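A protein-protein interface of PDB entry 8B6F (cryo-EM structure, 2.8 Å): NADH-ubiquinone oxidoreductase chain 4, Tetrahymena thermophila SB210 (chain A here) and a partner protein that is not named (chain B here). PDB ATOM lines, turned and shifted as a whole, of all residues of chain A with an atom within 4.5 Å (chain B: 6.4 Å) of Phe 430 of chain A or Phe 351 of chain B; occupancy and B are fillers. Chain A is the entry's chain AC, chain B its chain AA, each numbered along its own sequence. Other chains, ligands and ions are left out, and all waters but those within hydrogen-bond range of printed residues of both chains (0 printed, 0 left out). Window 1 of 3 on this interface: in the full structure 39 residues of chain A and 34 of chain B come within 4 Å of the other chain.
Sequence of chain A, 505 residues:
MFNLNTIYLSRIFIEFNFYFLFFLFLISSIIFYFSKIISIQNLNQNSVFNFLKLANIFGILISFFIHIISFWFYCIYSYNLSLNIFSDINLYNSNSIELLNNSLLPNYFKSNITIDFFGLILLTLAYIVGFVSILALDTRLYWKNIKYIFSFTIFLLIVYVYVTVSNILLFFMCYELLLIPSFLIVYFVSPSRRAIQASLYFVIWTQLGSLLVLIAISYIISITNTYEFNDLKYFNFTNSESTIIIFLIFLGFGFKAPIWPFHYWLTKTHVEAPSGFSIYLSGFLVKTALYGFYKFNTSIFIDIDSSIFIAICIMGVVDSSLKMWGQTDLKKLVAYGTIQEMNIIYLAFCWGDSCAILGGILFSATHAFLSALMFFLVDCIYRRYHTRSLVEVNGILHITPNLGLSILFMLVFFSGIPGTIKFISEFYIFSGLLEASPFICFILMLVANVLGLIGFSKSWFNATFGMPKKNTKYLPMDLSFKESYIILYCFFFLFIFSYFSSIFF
Phe 427 of chain A touches Phe 351 of chain B.
CE1 of Phe 427 of chain A touches CD2 of Leu 355 of chain B, 3.7 Å away.
CE2 of Phe 351 of chain B touches CD2 of Phe 430 of chain A (3.5 Å).
Ser 431 of chain A touches Leu 355 of chain B (OG to CD2, 3.4 Å).
O of Ser 431 of chain A touches OG of Ser 359 of chain B, at 3.9 Å.
Leu 434 of chain A touches Phe 352 of chain B.
Leu 355 of chain B touches Leu 434 of chain A (O to CD2, 3.4 Å).
CA of Ile 356 of chain B touches CD2 of Leu 434 of chain A, at 3.5 Å.
Met 445 of chain A touches Leu 348 of chain B (CB to CD1, 3.9 Å).
Met 445 of chain A touches Leu 355 of chain B.
Phe 430 of chain A touches just these residues of chain B: Phe 351 (3.5 Å) and Leu 355 (3.3 Å).
Of chain A, only Phe 427 (3.7 Å), Phe 430 (3.5 Å) and Met 445 (3.5 Å) come within 4 Å of Phe 351 of chain B.
Printed residues of chain A within 4 Å of Ser 359 of chain B: Ser 431 and Leu 434.
Of the printed residues of chain A, Leu 355 of chain B touches Phe 427 (3.7 Å), Phe 430 (3.3 Å), Ser 431 (3.4 Å), Leu 434 (3.4 Å) and Met 445 (3.5 Å).
Of the printed residues of chain A, Leu 348 of chain B touches Met 445 (3.9 Å).
The nearest residue of chain A that does not touch Phe 351 of chain B is Glu 426 of chain A (4.2 Å).
The nearest printed residue of chain B that does not touch Ser 431 of chain A is Phe 351 of chain B (6.3 Å).
Hydrophobic or aromatic side chains of chain B within 4 Å of the printed part of chain A: Phe 309, Leu 348, Phe 351, Phe 352, Leu 355 and Ile 356.
Of the 13 printed residues of chain A, 6 touch a printed residue of chain B.
Along chain A the printed residues that touch a printed residue of chain B span positions 423 to 445.
OG of Ser 359 of chain B sits at hydrogen-bond distance from O of Leu 355 of chain B (3.1 Å).
The side-chain hydroxyl (OG) of Ser 431 of chain A sits at hydrogen-bond distance from the backbone carbonyl oxygen (O) of Phe 427 of chain A (2.6 Å).
The backbone carbonyl oxygen of Phe 430 of chain A is in hydrogen-bond range of the side-chain sulfur of Cys 441 of chain A (3.6 Å).
SG of Cys 441 of chain A sits at hydrogen-bond distance from SD of Met 445 of chain A (3.7 Å).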
ATOM      1  N   PHE A 423     -16.522  36.342 -28.049  1.00  0.00           N
ATOM      2  CA  PHE A 423     -17.787  35.641 -27.869  1.00  0.00           C
ATOM      3  C   PHE A 423     -18.457  35.361 -29.208  1.00  0.00           C
ATOM      4  O   PHE A 423     -19.021  34.281 -29.413  1.00  0.00           O
ATOM      5  CB  PHE A 423     -18.719  36.458 -26.976  1.00  0.00           C
ATOM      6  CG  PHE A 423     -20.114  35.908 -26.896  1.00  0.00           C
ATOM      7  CD1 PHE A 423     -20.431  34.911 -25.990  1.00  0.00           C
ATOM      8  CD2 PHE A 423     -21.110  36.392 -27.730  1.00  0.00           C
ATOM      9  CE1 PHE A 423     -21.713  34.406 -25.918  1.00  0.00           C
ATOM     10  CE2 PHE A 423     -22.393  35.891 -27.663  1.00  0.00           C
ATOM     11  CZ  PHE A 423     -22.696  34.896 -26.755  1.00  0.00           C
ATOM     12  N   GLU A 426     -16.671  32.430 -30.884  1.00  0.00           N
ATOM     13  CA  GLU A 426     -17.044  31.196 -30.203  1.00  0.00           C
ATOM     14  C   GLU A 426     -18.459  30.782 -30.579  1.00  0.00           C
ATOM     15  O   GLU A 426     -18.729  29.597 -30.803  1.00  0.00           O
ATOM     16  CB  GLU A 426     -16.916  31.373 -28.692  1.00  0.00           C
ATOM     17  CG  GLU A 426     -15.477  31.409 -28.202  1.00  0.00           C
ATOM     18  CD  GLU A 426     -15.377  31.525 -26.693  1.00  0.00           C
ATOM     19  OE1 GLU A 426     -16.417  31.755 -26.041  1.00  0.00           O
ATOM     20  OE2 GLU A 426     -14.258  31.386 -26.157  1.00  0.00           O
ATOM     21  N   PHE A 427     -19.375  31.748 -30.656  1.00  0.00           N
ATOM     22  CA  PHE A 427     -20.753  31.437 -31.016  1.00  0.00           C
ATOM     23  C   PHE A 427     -20.828  30.851 -32.422  1.00  0.00           C
ATOM     24  O   PHE A 427     -21.503  29.840 -32.647  1.00  0.00           O
ATOM     25  CB  PHE A 427     -21.609  32.698 -30.906  1.00  0.00           C
ATOM     26  CG  PHE A 427     -23.081  32.425 -30.814  1.00  0.00           C
ATOM     27  CD1 PHE A 427     -23.669  32.162 -29.587  1.00  0.00           C
ATOM     28  CD2 PHE A 427     -23.879  32.444 -31.944  1.00  0.00           C
ATOM     29  CE1 PHE A 427     -25.023  31.915 -29.490  1.00  0.00           C
ATOM     30  CE2 PHE A 427     -25.235  32.198 -31.853  1.00  0.00           C
ATOM     31  CZ  PHE A 427     -25.807  31.933 -30.624  1.00  0.00           C
ATOM     32  N   TYR A 428     -20.147  31.478 -33.385  1.00  0.00           N
ATOM     33  CA  TYR A 428     -20.132  30.944 -34.745  1.00  0.00           C
ATOM     34  C   TYR A 428     -19.629  29.506 -34.765  1.00  0.00           C
ATOM     35  O   TYR A 428     -20.287  28.611 -35.303  1.00  0.00           O
ATOM     36  CB  TYR A 428     -19.239  31.806 -35.638  1.00  0.00           C
ATOM     37  CG  TYR A 428     -19.919  32.959 -36.339  1.00  0.00           C
ATOM     38  CD1 TYR A 428     -20.192  34.144 -35.671  1.00  0.00           C
ATOM     39  CD2 TYR A 428     -20.239  32.877 -37.687  1.00  0.00           C
ATOM     40  CE1 TYR A 428     -20.792  35.203 -36.317  1.00  0.00           C
ATOM     41  CE2 TYR A 428     -20.839  33.932 -38.342  1.00  0.00           C
ATOM     42  CZ  TYR A 428     -21.113  35.093 -37.652  1.00  0.00           C
ATOM     43  OH  TYR A 428     -21.710  36.148 -38.299  1.00  0.00           O
ATOM     44  N   ILE A 429     -18.448  29.274 -34.190  1.00  0.00           N
ATOM     45  CA  ILE A 429     -17.808  27.967 -34.305  1.00  0.00           C
ATOM     46  C   ILE A 429     -18.635  26.903 -33.602  1.00  0.00           C
ATOM     47  O   ILE A 429     -18.843  25.805 -34.130  1.00  0.00           O
ATOM     48  CB  ILE A 429     -16.372  28.028 -33.748  1.00  0.00           C
ATOM     49  CG1 ILE A 429     -15.529  29.037 -34.534  1.00  0.00           C
ATOM     50  CG2 ILE A 429     -15.722  26.649 -33.774  1.00  0.00           C
ATOM     51  CD1 ILE A 429     -15.414  28.742 -36.014  1.00  0.00           C
ATOM     52  N   PHE A 430     -19.118  27.208 -32.397  1.00  0.00           N
ATOM     53  CA  PHE A 430     -19.877  26.224 -31.639  1.00  0.00           C
ATOM     54  C   PHE A 430     -21.251  25.980 -32.243  1.00  0.00           C
ATOM     55  O   PHE A 430     -21.751  24.851 -32.194  1.00  0.00           O
ATOM     56  CB  PHE A 430     -20.003  26.670 -30.181  1.00  0.00           C
ATOM     57  CG  PHE A 430     -18.683  26.885 -29.491  1.00  0.00           C
ATOM     58  CD1 PHE A 430     -17.533  26.254 -29.939  1.00  0.00           C
ATOM     59  CD2 PHE A 430     -18.597  27.715 -28.387  1.00  0.00           C
ATOM     60  CE1 PHE A 430     -16.323  26.452 -29.301  1.00  0.00           C
ATOM     61  CE2 PHE A 430     -17.389  27.917 -27.746  1.00  0.00           C
ATOM     62  CZ  PHE A 430     -16.253  27.284 -28.203  1.00  0.00           C
ATOM     63  N   SER A 431     -21.881  27.009 -32.813  1.00  0.00           N
ATOM     64  CA  SER A 431     -23.159  26.791 -33.480  1.00  0.00           C
ATOM     65  C   SER A 431     -23.007  25.841 -34.659  1.00  0.00           C
ATOM     66  O   SER A 431     -23.853  24.966 -34.874  1.00  0.00           O
ATOM     67  CB  SER A 431     -23.738  28.125 -33.949  1.00  0.00           C
ATOM     68  OG  SER A 431     -23.951  29.002 -32.857  1.00  0.00           O
ATOM     69  N   GLY A 432     -21.946  26.006 -35.446  1.00  0.00           N
ATOM     70  CA  GLY A 432     -21.689  25.068 -36.524  1.00  0.00           C
ATOM     71  C   GLY A 432     -21.336  23.681 -36.024  1.00  0.00           C
ATOM     72  O   GLY A 432     -21.835  22.679 -36.543  1.00  0.00           O
ATOM     73  N   LEU A 433     -20.467  23.601 -35.011  1.00  0.00           N
ATOM     74  CA  LEU A 433     -20.001  22.304 -34.532  1.00  0.00           C
ATOM     75  C   LEU A 433     -21.108  21.522 -33.843  1.00  0.00           C
ATOM     76  O   LEU A 433     -21.064  20.288 -33.816  1.00  0.00           O
ATOM     77  CB  LEU A 433     -18.823  22.480 -33.576  1.00  0.00           C
ATOM     78  CG  LEU A 433     -17.461  22.810 -34.189  1.00  0.00           C
ATOM     79  CD1 LEU A 433     -16.444  23.088 -33.096  1.00  0.00           C
ATOM     80  CD2 LEU A 433     -16.979  21.678 -35.075  1.00  0.00           C
ATOM     81  N   LEU A 434     -22.097  22.213 -33.276  1.00  0.00           N
ATOM     82  CA  LEU A 434     -23.193  21.506 -32.627  1.00  0.00           C
ATOM     83  C   LEU A 434     -23.957  20.656 -33.631  1.00  0.00           C
ATOM     84  O   LEU A 434     -24.313  19.508 -33.341  1.00  0.00           O
ATOM     85  CB  LEU A 434     -24.122  22.500 -31.930  1.00  0.00           C
ATOM     86  CG  LEU A 434     -25.255  21.887 -31.105  1.00  0.00           C
ATOM     87  CD1 LEU A 434     -24.717  21.037 -29.971  1.00  0.00           C
ATOM     88  CD2 LEU A 434     -26.135  22.970 -30.542  1.00  0.00           C
ATOM     89  N   CYS A 441     -18.629  18.801 -30.118  1.00  0.00           N
ATOM     90  CA  CYS A 441     -18.772  20.195 -29.718  1.00  0.00           C
ATOM     91  C   CYS A 441     -18.841  20.322 -28.203  1.00  0.00           C
ATOM     92  O   CYS A 441     -18.219  21.218 -27.621  1.00  0.00           O
ATOM     93  CB  CYS A 441     -20.018  20.800 -30.363  1.00  0.00           C
ATOM     94  SG  CYS A 441     -20.337  22.510 -29.888  1.00  0.00           S
ATOM     95  N   MET A 445     -16.057  22.383 -26.055  1.00  0.00           N
ATOM     96  CA  MET A 445     -16.463  23.501 -25.210  1.00  0.00           C
ATOM     97  C   MET A 445     -16.113  23.237 -23.753  1.00  0.00           C
ATOM     98  O   MET A 445     -15.511  24.083 -23.085  1.00  0.00           O
ATOM     99  CB  MET A 445     -17.962  23.761 -25.359  1.00  0.00           C
ATOM    100  CG  MET A 445     -18.361  24.319 -26.712  1.00  0.00           C
ATOM    101  SD  MET A 445     -20.126  24.667 -26.830  1.00  0.00           S
ATOM    102  CE  MET A 445     -20.325  25.896 -25.539  1.00  0.00           C
ATOM    103  N   ASN A 449     -13.286  25.772 -22.344  1.00  0.00           N
ATOM    104  CA  ASN A 449     -13.876  26.862 -21.581  1.00  0.00           C
ATOM    105  C   ASN A 449     -14.046  26.557 -20.099  1.00  0.00           C
ATOM    106  O   ASN A 449     -14.536  27.421 -19.366  1.00  0.00           O
ATOM    107  CB  ASN A 449     -15.237  27.242 -22.171  1.00  0.00           C
ATOM    108  CG  ASN A 449     -15.136  27.724 -23.603  1.00  0.00           C
ATOM    109  OD1 ASN A 449     -14.060  28.095 -24.069  1.00  0.00           O
ATOM    110  ND2 ASN A 449     -16.262  27.736 -24.304  1.00  0.00           N
ATOM    111  N   PHE B 309     -27.306  35.553 -20.857  1.00  0.00           N
ATOM    112  CA  PHE B 309     -25.965  35.013 -20.661  1.00  0.00           C
ATOM    113  C   PHE B 309     -24.998  36.098 -20.211  1.00  0.00           C
ATOM    114  O   PHE B 309     -24.137  35.854 -19.360  1.00  0.00           O
ATOM    115  CB  PHE B 309     -25.479  34.350 -21.949  1.00  0.00           C
ATOM    116  CG  PHE B 309     -24.207  33.567 -21.787  1.00  0.00           C
ATOM    117  CD1 PHE B 309     -24.219  32.321 -21.187  1.00  0.00           C
ATOM    118  CD2 PHE B 309     -23.006  34.069 -22.251  1.00  0.00           C
ATOM    119  CE1 PHE B 309     -23.054  31.595 -21.041  1.00  0.00           C
ATOM    120  CE2 PHE B 309     -21.836  33.348 -22.109  1.00  0.00           C
ATOM    121  CZ  PHE B 309     -21.861  32.110 -21.504  1.00  0.00           C
ATOM    122  N   SER B 346     -21.279  26.527 -14.686  1.00  0.00           N
ATOM    123  CA  SER B 346     -22.652  26.923 -14.979  1.00  0.00           C
ATOM    124  C   SER B 346     -22.727  27.702 -16.285  1.00  0.00           C
ATOM    125  O   SER B 346     -23.671  27.537 -17.065  1.00  0.00           O
ATOM    126  CB  SER B 346     -23.225  27.747 -13.825  1.00  0.00           C
ATOM    127  OG  SER B 346     -22.594  29.009 -13.728  1.00  0.00           O
ATOM    128  N   ASP B 347     -21.736  28.559 -16.540  1.00  0.00           N
ATOM    129  CA  ASP B 347     -21.693  29.290 -17.801  1.00  0.00           C
ATOM    130  C   ASP B 347     -21.580  28.338 -18.983  1.00  0.00           C
ATOM    131  O   ASP B 347     -22.236  28.534 -20.011  1.00  0.00           O
ATOM    132  CB  ASP B 347     -20.520  30.273 -17.801  1.00  0.00           C
ATOM    133  CG  ASP B 347     -20.611  31.291 -16.684  1.00  0.00           C
ATOM    134  OD1 ASP B 347     -21.555  31.201 -15.873  1.00  0.00           O
ATOM    135  OD2 ASP B 347     -19.737  32.179 -16.611  1.00  0.00           O
ATOM    136  N   LEU B 348     -20.747  27.304 -18.859  1.00  0.00           N
ATOM    137  CA  LEU B 348     -20.658  26.301 -19.915  1.00  0.00           C
ATOM    138  C   LEU B 348     -22.018  25.675 -20.190  1.00  0.00           C
ATOM    139  O   LEU B 348     -22.444  25.573 -21.345  1.00  0.00           O
ATOM    140  CB  LEU B 348     -19.644  25.224 -19.524  1.00  0.00           C
ATOM    141  CG  LEU B 348     -19.754  23.886 -20.262  1.00  0.00           C
ATOM    142  CD1 LEU B 348     -19.478  24.068 -21.743  1.00  0.00           C
ATOM    143  CD2 LEU B 348     -18.813  22.865 -19.661  1.00  0.00           C
ATOM    144  N   PHE B 349     -22.715  25.238 -19.139  1.00  0.00           N
ATOM    145  CA  PHE B 349     -24.008  24.593 -19.337  1.00  0.00           C
ATOM    146  C   PHE B 349     -24.991  25.546 -20.005  1.00  0.00           C
ATOM    147  O   PHE B 349     -25.698  25.169 -20.945  1.00  0.00           O
ATOM    148  CB  PHE B 349     -24.561  24.103 -17.996  1.00  0.00           C
ATOM    149  CG  PHE B 349     -23.814  22.932 -17.414  1.00  0.00           C
ATOM    150  CD1 PHE B 349     -23.147  22.031 -18.227  1.00  0.00           C
ATOM    151  CD2 PHE B 349     -23.787  22.733 -16.045  1.00  0.00           C
ATOM    152  CE1 PHE B 349     -22.467  20.961 -17.686  1.00  0.00           C
ATOM    153  CE2 PHE B 349     -23.108  21.665 -15.501  1.00  0.00           C
ATOM    154  CZ  PHE B 349     -22.447  20.778 -16.322  1.00  0.00           C
ATOM    155  N   LEU B 350     -25.046  26.791 -19.529  1.00  0.00           N
ATOM    156  CA  LEU B 350     -25.984  27.755 -20.091  1.00  0.00           C
ATOM    157  C   LEU B 350     -25.654  28.055 -21.547  1.00  0.00           C
ATOM    158  O   LEU B 350     -26.553  28.146 -22.391  1.00  0.00           O
ATOM    159  CB  LEU B 350     -25.974  29.038 -19.260  1.00  0.00           C
ATOM    160  CG  LEU B 350     -26.992  30.114 -19.644  1.00  0.00           C
ATOM    161  CD1 LEU B 350     -28.415  29.606 -19.496  1.00  0.00           C
ATOM    162  CD2 LEU B 350     -26.787  31.356 -18.800  1.00  0.00           C
ATOM    163  N   PHE B 351     -24.366  28.206 -21.862  1.00  0.00           N
ATOM    164  CA  PHE B 351     -23.966  28.474 -23.238  1.00  0.00           C
ATOM    165  C   PHE B 351     -24.345  27.319 -24.155  1.00  0.00           C
ATOM    166  O   PHE B 351     -24.837  27.537 -25.267  1.00  0.00           O
ATOM    167  CB  PHE B 351     -22.460  28.737 -23.296  1.00  0.00           C
ATOM    168  CG  PHE B 351     -21.969  29.261 -24.624  1.00  0.00           C
ATOM    169  CD1 PHE B 351     -22.852  29.657 -25.618  1.00  0.00           C
ATOM    170  CD2 PHE B 351     -20.611  29.352 -24.875  1.00  0.00           C
ATOM    171  CE1 PHE B 351     -22.387  30.134 -26.828  1.00  0.00           C
ATOM    172  CE2 PHE B 351     -20.143  29.828 -26.082  1.00  0.00           C
ATOM    173  CZ  PHE B 351     -21.031  30.219 -27.060  1.00  0.00           C
ATOM    174  N   PHE B 352     -24.125  26.083 -23.705  1.00  0.00           N
ATOM    175  CA  PHE B 352     -24.476  24.933 -24.530  1.00  0.00           C
ATOM    176  C   PHE B 352     -25.981  24.848 -24.747  1.00  0.00           C
ATOM    177  O   PHE B 352     -26.439  24.540 -25.853  1.00  0.00           O
ATOM    178  CB  PHE B 352     -23.948  23.647 -23.896  1.00  0.00           C
ATOM    179  CG  PHE B 352     -23.798  22.516 -24.870  1.00  0.00           C
ATOM    180  CD1 PHE B 352     -22.755  22.504 -25.779  1.00  0.00           C
ATOM    181  CD2 PHE B 352     -24.707  21.475 -24.888  1.00  0.00           C
ATOM    182  CE1 PHE B 352     -22.617  21.470 -26.682  1.00  0.00           C
ATOM    183  CE2 PHE B 352     -24.574  20.436 -25.790  1.00  0.00           C
ATOM    184  CZ  PHE B 352     -23.528  20.434 -26.687  1.00  0.00           C
ATOM    185  N   ALA B 353     -26.769  25.121 -23.706  1.00  0.00           N
ATOM    186  CA  ALA B 353     -28.221  25.113 -23.860  1.00  0.00           C
ATOM    187  C   ALA B 353     -28.674  26.173 -24.856  1.00  0.00           C
ATOM    188  O   ALA B 353     -29.546  25.918 -25.694  1.00  0.00           O
ATOM    189  CB  ALA B 353     -28.893  25.332 -22.506  1.00  0.00           C
ATOM    190  N   ILE B 354     -28.094  27.372 -24.776  1.00  0.00           N
ATOM    191  CA  ILE B 354     -28.450  28.438 -25.708  1.00  0.00           C
ATOM    192  C   ILE B 354     -28.073  28.048 -27.130  1.00  0.00           C
ATOM    193  O   ILE B 354     -28.808  28.334 -28.083  1.00  0.00           O
ATOM    194  CB  ILE B 354     -27.784  29.760 -25.281  1.00  0.00           C
ATOM    195  CG1 ILE B 354     -28.330  30.209 -23.924  1.00  0.00           C
ATOM    196  CG2 ILE B 354     -28.016  30.841 -26.328  1.00  0.00           C
ATOM    197  CD1 ILE B 354     -27.515  31.299 -23.263  1.00  0.00           C
ATOM    198  N   LEU B 355     -26.922  27.397 -27.301  1.00  0.00           N
ATOM    199  CA  LEU B 355     -26.520  26.949 -28.630  1.00  0.00           C
ATOM    200  C   LEU B 355     -27.499  25.920 -29.181  1.00  0.00           C
ATOM    201  O   LEU B 355     -27.842  25.955 -30.368  1.00  0.00           O
ATOM    202  CB  LEU B 355     -25.106  26.373 -28.588  1.00  0.00           C
ATOM    203  CG  LEU B 355     -23.966  27.371 -28.377  1.00  0.00           C
ATOM    204  CD1 LEU B 355     -22.664  26.624 -28.202  1.00  0.00           C
ATOM    205  CD2 LEU B 355     -23.860  28.358 -29.527  1.00  0.00           C
ATOM    206  N   ILE B 356     -27.950  24.988 -28.340  1.00  0.00           N
ATOM    207  CA  ILE B 356     -28.940  24.012 -28.787  1.00  0.00           C
ATOM    208  C   ILE B 356     -30.217  24.720 -29.216  1.00  0.00           C
ATOM    209  O   ILE B 356     -30.804  24.398 -30.255  1.00  0.00           O
ATOM    210  CB  ILE B 356     -29.211  22.978 -27.678  1.00  0.00           C
ATOM    211  CG1 ILE B 356     -27.962  22.132 -27.421  1.00  0.00           C
ATOM    212  CG2 ILE B 356     -30.380  22.076 -28.059  1.00  0.00           C
ATOM    213  CD1 ILE B 356     -28.071  21.233 -26.207  1.00  0.00           C
ATOM    214  N   SER B 359     -29.668  26.428 -32.581  1.00  0.00           N
ATOM    215  CA  SER B 359     -29.618  25.465 -33.676  1.00  0.00           C
ATOM    216  C   SER B 359     -31.008  24.952 -34.027  1.00  0.00           C
ATOM    217  O   SER B 359     -31.340  24.796 -35.208  1.00  0.00           O
ATOM    218  CB  SER B 359     -28.687  24.305 -33.327  1.00  0.00           C
ATOM    219  OG  SER B 359     -27.350  24.759 -33.201  1.00  0.00           O
